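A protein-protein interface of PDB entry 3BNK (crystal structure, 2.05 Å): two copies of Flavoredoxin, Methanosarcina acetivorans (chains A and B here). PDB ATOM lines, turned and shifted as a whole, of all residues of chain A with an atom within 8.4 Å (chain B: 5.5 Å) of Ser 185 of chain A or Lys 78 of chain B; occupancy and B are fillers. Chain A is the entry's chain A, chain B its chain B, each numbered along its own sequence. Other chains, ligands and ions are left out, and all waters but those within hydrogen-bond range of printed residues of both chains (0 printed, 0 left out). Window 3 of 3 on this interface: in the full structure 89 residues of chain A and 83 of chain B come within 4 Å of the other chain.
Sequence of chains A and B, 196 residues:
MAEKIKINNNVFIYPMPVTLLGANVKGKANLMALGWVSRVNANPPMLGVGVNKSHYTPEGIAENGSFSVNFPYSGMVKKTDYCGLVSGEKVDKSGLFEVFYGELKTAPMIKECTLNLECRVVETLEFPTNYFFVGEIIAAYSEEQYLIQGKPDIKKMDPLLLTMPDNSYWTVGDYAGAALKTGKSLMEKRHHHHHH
Among the printed residues, pairs that only touch across the chains: Ala 178 of chain A with Asp 81 of chain B (3.8 Å), Thr 182 of chain A with Lys 78 of chain B (3.4 Å), Gly 183 of chain A with Lys 78 of chain B (3.5 Å), Gly 183 of chain A with Tyr 82 of chain B (3.6 Å), Ser 185 of chain A with Lys 78 of chain B (3.8 Å), Leu 186 of chain A with Lys 79 of chain B (3.6 Å), Leu 186 of chain A with Tyr 82 of chain B (3.8 Å) and Met 187 of chain A with Tyr 82 of chain B (3.5 Å).
Of the 9 printed residues of chain B, 4 touch a printed residue of chain A. Along chain B the printed residues that touch a printed residue of chain A span positions 78 to 82. Among the printed residues, no Asp or Glu carboxylate lies within 4 Å of a Lys or Arg side-chain nitrogen of the other chain.
The backbone carbonyl oxygen (O) of Lys 79 of chain B lies within hydrogen-bond range of the side-chain sulfur (SG) of Cys 83 of chain B, 3.5 Å away. O of Ala 178 of chain A sits at hydrogen-bond distance from OG1 of Thr 182 of chain A, at 3.2 Å. The side-chain hydroxyl (OG) of Ser 185 of chain A sits at hydrogen-bond distance from the backbone carbonyl oxygen (O) of Thr 182 of chain A (3.1 Å).
The backbone NH (N) of Thr 182 of chain A sits at hydrogen-bond distance from the side-chain carboxylate (OD2) of Asp 81 of chain B, at 3.3 Å. The backbone NH (N) of Gly 183 of chain A is in hydrogen-bond range of the side-chain carboxylate (OD2) of Asp 81 of chain B, at 2.9 Å. N of Lys 181 of chain A is in hydrogen-bond range of OD2 of Asp 81 of chain B (2.9 Å).
No position is printed for both chains. Of the 11 pairs that touch across the chains among the printed residues, none has its exchanged pair printed and touching as well.
Ala 176 of chain A touches none of the printed residues of chain B. Of the printed residues of chain B, Ala 178 of chain A touches Asp 81 (3.8 Å). Of the printed residues of chain B, Lys 181 of chain A touches Asp 81. Of chain B, only Lys 78 (3.8 Å) comes within 4 Å of Ser 185 of chain A. Printed residues of chain B within 4 Å of Met 187 of chain A: Tyr 82 (3.5 Å). Of the printed residues of chain A, Lys 78 of chain B touches Thr 182 (3.4 Å), Gly 183 (3.5 Å) and Ser 185 (3.8 Å). Of the printed residues of chain A, Lys 79 of chain B touches Leu 186 (3.6 Å). Printed residues of chain A within 4 Å of Asp 81 of chain B: Ala 178 (3.8 Å), Lys 181 (2.9 Å), Thr 182 (3.3 Å) and Gly 183 (2.9 Å). The nearest residue of chain A that does not touch Lys 78 of chain B is Leu 186 of chain A (4.1 Å).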
ATOM      1  N   ALA A 176      20.718   6.426 -17.674  1.00  0.00           N
ATOM      2  CA  ALA A 176      22.049   6.996 -17.530  1.00  0.00           C
ATOM      3  C   ALA A 176      22.027   8.476 -17.154  1.00  0.00           C
ATOM      4  O   ALA A 176      23.061   9.138 -17.194  1.00  0.00           O
ATOM      5  CB  ALA A 176      22.874   6.765 -18.821  1.00  0.00           C
ATOM      6  N   GLY A 177      20.857   9.000 -16.800  1.00  0.00           N
ATOM      7  CA  GLY A 177      20.752  10.404 -16.393  1.00  0.00           C
ATOM      8  C   GLY A 177      19.587  11.171 -16.992  1.00  0.00           C
ATOM      9  O   GLY A 177      18.908  10.692 -17.913  1.00  0.00           O
ATOM     10  N   ALA A 178      19.357  12.367 -16.448  1.00  0.00           N
ATOM     11  CA  ALA A 178      18.290  13.248 -16.909  1.00  0.00           C
ATOM     12  C   ALA A 178      18.854  14.214 -17.941  1.00  0.00           C
ATOM     13  O   ALA A 178      19.786  14.963 -17.641  1.00  0.00           O
ATOM     14  CB  ALA A 178      17.689  14.006 -15.739  1.00  0.00           C
ATOM     15  N   LYS A 181      19.277  18.514 -17.830  1.00  0.00           N
ATOM     16  CA  LYS A 181      19.272  18.612 -16.364  1.00  0.00           C
ATOM     17  C   LYS A 181      20.641  18.303 -15.725  1.00  0.00           C
ATOM     18  O   LYS A 181      21.207  19.168 -15.053  1.00  0.00           O
ATOM     19  CB  LYS A 181      18.168  17.734 -15.750  1.00  0.00           C
ATOM     20  CG  LYS A 181      17.809  18.102 -14.303  1.00  0.00           C
ATOM     21  CD  LYS A 181      17.024  17.004 -13.568  1.00  0.00           C
ATOM     22  CE  LYS A 181      15.629  16.802 -14.159  1.00  0.00           C
ATOM     23  NZ  LYS A 181      14.700  16.036 -13.272  1.00  0.00           N
ATOM     24  N   THR A 182      21.173  17.093 -15.938  1.00  0.00           N
ATOM     25  CA  THR A 182      22.447  16.700 -15.304  1.00  0.00           C
ATOM     26  C   THR A 182      23.588  17.670 -15.593  1.00  0.00           C
ATOM     27  O   THR A 182      24.454  17.873 -14.745  1.00  0.00           O
ATOM     28  CB  THR A 182      22.899  15.257 -15.672  1.00  0.00           C
ATOM     29  OG1 THR A 182      21.866  14.326 -15.343  1.00  0.00           O
ATOM     30  CG2 THR A 182      24.152  14.859 -14.910  1.00  0.00           C
ATOM     31  N   GLY A 183      23.581  18.268 -16.784  1.00  0.00           N
ATOM     32  CA  GLY A 183      24.611  19.213 -17.186  1.00  0.00           C
ATOM     33  C   GLY A 183      24.535  20.578 -16.518  1.00  0.00           C
ATOM     34  O   GLY A 183      25.421  21.416 -16.732  1.00  0.00           O
ATOM     35  N   LYS A 184      23.487  20.804 -15.718  1.00  0.00           N
ATOM     36  CA  LYS A 184      23.295  22.080 -15.002  1.00  0.00           C
ATOM     37  C   LYS A 184      24.443  22.372 -14.021  1.00  0.00           C
ATOM     38  O   LYS A 184      24.742  23.527 -13.746  1.00  0.00           O
ATOM     39  CB  LYS A 184      21.943  22.124 -14.264  1.00  0.00           C
ATOM     40  CG  LYS A 184      20.700  22.076 -15.157  1.00  0.00           C
ATOM     41  CD  LYS A 184      20.038  23.446 -15.325  1.00  0.00           C
ATOM     42  CE  LYS A 184      19.119  23.494 -16.563  1.00  0.00           C
ATOM     43  NZ  LYS A 184      19.022  24.869 -17.153  1.00  0.00           N
ATOM     44  N   SER A 185      25.089  21.317 -13.522  1.00  0.00           N
ATOM     45  CA  SER A 185      26.228  21.441 -12.594  1.00  0.00           C
ATOM     46  C   SER A 185      27.440  22.203 -13.153  1.00  0.00           C
ATOM     47  O   SER A 185      28.150  22.884 -12.403  1.00  0.00           O
ATOM     48  CB  SER A 185      26.657  20.062 -12.068  1.00  0.00           C
ATOM     49  OG  SER A 185      26.739  19.091 -13.105  1.00  0.00           O
ATOM     50  N   LEU A 186      27.659  22.096 -14.465  1.00  0.00           N
ATOM     51  CA  LEU A 186      28.812  22.729 -15.123  1.00  0.00           C
ATOM     52  C   LEU A 186      28.631  24.229 -15.374  1.00  0.00           C
ATOM     53  O   LEU A 186      29.553  24.890 -15.848  1.00  0.00           O
ATOM     54  CB  LEU A 186      29.155  22.024 -16.446  1.00  0.00           C
ATOM     55  CG  LEU A 186      29.452  20.521 -16.532  1.00  0.00           C
ATOM     56  CD1 LEU A 186      30.273  20.253 -17.775  1.00  0.00           C
ATOM     57  CD2 LEU A 186      30.178  19.986 -15.313  1.00  0.00           C
ATOM     58  N   MET A 187      27.440  24.749 -15.070  1.00  0.00           N
ATOM     59  CA  MET A 187      27.129  26.175 -15.233  1.00  0.00           C
ATOM     60  C   MET A 187      27.725  27.008 -14.093  1.00  0.00           C
ATOM     61  O   MET A 187      27.280  26.954 -12.943  1.00  0.00           O
ATOM     62  CB  MET A 187      25.605  26.394 -15.351  1.00  0.00           C
ATOM     63  CG  MET A 187      24.986  25.779 -16.617  1.00  0.00           C
ATOM     64  SD  MET A 187      23.177  25.678 -16.701  1.00  0.00           S
ATOM     65  CE  MET A 187      22.764  27.338 -17.264  1.00  0.00           C
ATOM     66  N   GLY B  75      30.487   8.225 -19.705  1.00  0.00           N
ATOM     67  CA  GLY B  75      31.094   9.048 -18.648  1.00  0.00           C
ATOM     68  C   GLY B  75      31.216  10.534 -18.965  1.00  0.00           C
ATOM     69  O   GLY B  75      31.523  11.329 -18.082  1.00  0.00           O
ATOM     70  N   MET B  76      30.977  10.918 -20.219  1.00  0.00           N
ATOM     71  CA  MET B  76      30.948  12.342 -20.598  1.00  0.00           C
ATOM     72  C   MET B  76      29.536  12.944 -20.556  1.00  0.00           C
ATOM     73  O   MET B  76      29.330  14.059 -21.066  1.00  0.00           O
ATOM     74  CB  MET B  76      31.528  12.543 -21.998  1.00  0.00           C
ATOM     75  CG  MET B  76      32.993  12.191 -22.169  1.00  0.00           C
ATOM     76  SD  MET B  76      33.466  12.143 -23.919  1.00  0.00           S
ATOM     77  CE  MET B  76      33.271  13.879 -24.352  1.00  0.00           C
ATOM     78  N   VAL B  77      28.575  12.221 -19.965  1.00  0.00           N
ATOM     79  CA  VAL B  77      27.164  12.665 -19.902  1.00  0.00           C
ATOM     80  C   VAL B  77      26.984  14.144 -19.559  1.00  0.00           C
ATOM     81  O   VAL B  77      26.275  14.847 -20.272  1.00  0.00           O
ATOM     82  CB  VAL B  77      26.247  11.791 -18.948  1.00  0.00           C
ATOM     83  CG1 VAL B  77      26.193  10.361 -19.411  1.00  0.00           C
ATOM     84  CG2 VAL B  77      26.699  11.828 -17.481  1.00  0.00           C
ATOM     85  N   LYS B  78      27.651  14.611 -18.499  1.00  0.00           N
ATOM     86  CA  LYS B  78      27.484  15.984 -18.001  1.00  0.00           C
ATOM     87  C   LYS B  78      27.952  17.081 -18.956  1.00  0.00           C
ATOM     88  O   LYS B  78      27.188  17.997 -19.252  1.00  0.00           O
ATOM     89  CB  LYS B  78      28.140  16.167 -16.627  1.00  0.00           C
ATOM     90  CG  LYS B  78      27.399  15.462 -15.507  1.00  0.00           C
ATOM     91  CD  LYS B  78      28.063  15.675 -14.160  1.00  0.00           C
ATOM     92  CE  LYS B  78      27.514  14.717 -13.114  1.00  0.00           C
ATOM     93  NZ  LYS B  78      28.644  14.232 -12.230  1.00  0.00           N
ATOM     94  N   LYS B  79      29.202  16.997 -19.419  1.00  0.00           N
ATOM     95  CA  LYS B  79      29.726  17.937 -20.430  1.00  0.00           C
ATOM     96  C   LYS B  79      28.838  17.955 -21.670  1.00  0.00           C
ATOM     97  O   LYS B  79      28.539  19.029 -22.213  1.00  0.00           O
ATOM     98  CB  LYS B  79      31.159  17.579 -20.835  1.00  0.00           C
ATOM     99  CG  LYS B  79      32.251  18.113 -19.934  1.00  0.00           C
ATOM    100  CD  LYS B  79      33.628  17.917 -20.564  1.00  0.00           C
ATOM    101  CE  LYS B  79      34.744  18.486 -19.670  1.00  0.00           C
ATOM    102  NZ  LYS B  79      36.106  18.183 -20.212  1.00  0.00           N
ATOM    103  N   THR B  80      28.418  16.762 -22.098  1.00  0.00           N
ATOM    104  CA  THR B  80      27.507  16.598 -23.232  1.00  0.00           C
ATOM    105  C   THR B  80      26.194  17.355 -23.012  1.00  0.00           C
ATOM    106  O   THR B  80      25.811  18.195 -23.833  1.00  0.00           O
ATOM    107  CB  THR B  80      27.214  15.097 -23.539  1.00  0.00           C
ATOM    108  OG1 THR B  80      28.440  14.411 -23.803  1.00  0.00           O
ATOM    109  CG2 THR B  80      26.290  14.956 -24.756  1.00  0.00           C
ATOM    110  N   ASP B  81      25.527  17.063 -21.896  1.00  0.00           N
ATOM    111  CA  ASP B  81      24.252  17.696 -21.558  1.00  0.00           C
ATOM    112  C   ASP B  81      24.382  19.221 -21.444  1.00  0.00           C
ATOM    113  O   ASP B  81      23.514  19.968 -21.920  1.00  0.00           O
ATOM    114  CB  ASP B  81      23.712  17.105 -20.263  1.00  0.00           C
ATOM    115  CG  ASP B  81      22.230  17.306 -20.111  1.00  0.00           C
ATOM    116  OD1 ASP B  81      21.470  16.956 -21.045  1.00  0.00           O
ATOM    117  OD2 ASP B  81      21.828  17.825 -19.052  1.00  0.00           O
ATOM    118  N   TYR B  82      25.485  19.663 -20.836  1.00  0.00           N
ATOM    119  CA  TYR B  82      25.842  21.068 -20.711  1.00  0.00           C
ATOM    120  C   TYR B  82      25.889  21.781 -22.060  1.00  0.00           C
ATOM    121  O   TYR B  82      25.473  22.933 -22.177  1.00  0.00           O
ATOM    122  CB  TYR B  82      27.186  21.211 -19.990  1.00  0.00           C
ATOM    123  CG  TYR B  82      27.675  22.647 -19.878  1.00  0.00           C
ATOM    124  CD1 TYR B  82      26.984  23.578 -19.084  1.00  0.00           C
ATOM    125  CD2 TYR B  82      28.823  23.078 -20.562  1.00  0.00           C
ATOM    126  CE1 TYR B  82      27.418  24.889 -18.970  1.00  0.00           C
ATOM    127  CE2 TYR B  82      29.270  24.408 -20.452  1.00  0.00           C
ATOM    128  CZ  TYR B  82      28.550  25.303 -19.658  1.00  0.00           C
ATOM    129  OH  TYR B  82      28.961  26.608 -19.517  1.00  0.00           O
ATOM    130  N   CYS B  83      26.406  21.084 -23.069  1.00  0.00           N
ATOM    131  CA  CYS B  83      26.446  21.579 -24.441  1.00  0.00           C
ATOM    132  C   CYS B  83      25.061  21.676 -25.073  1.00  0.00           C
ATOM    133  O   CYS B  83      24.888  22.381 -26.058  1.00  0.00           O
ATOM    134  CB  CYS B  83      27.349  20.682 -25.293  1.00  0.00           C
ATOM    135  SG  CYS B  83      29.076  21.039 -25.010  1.00  0.00           S
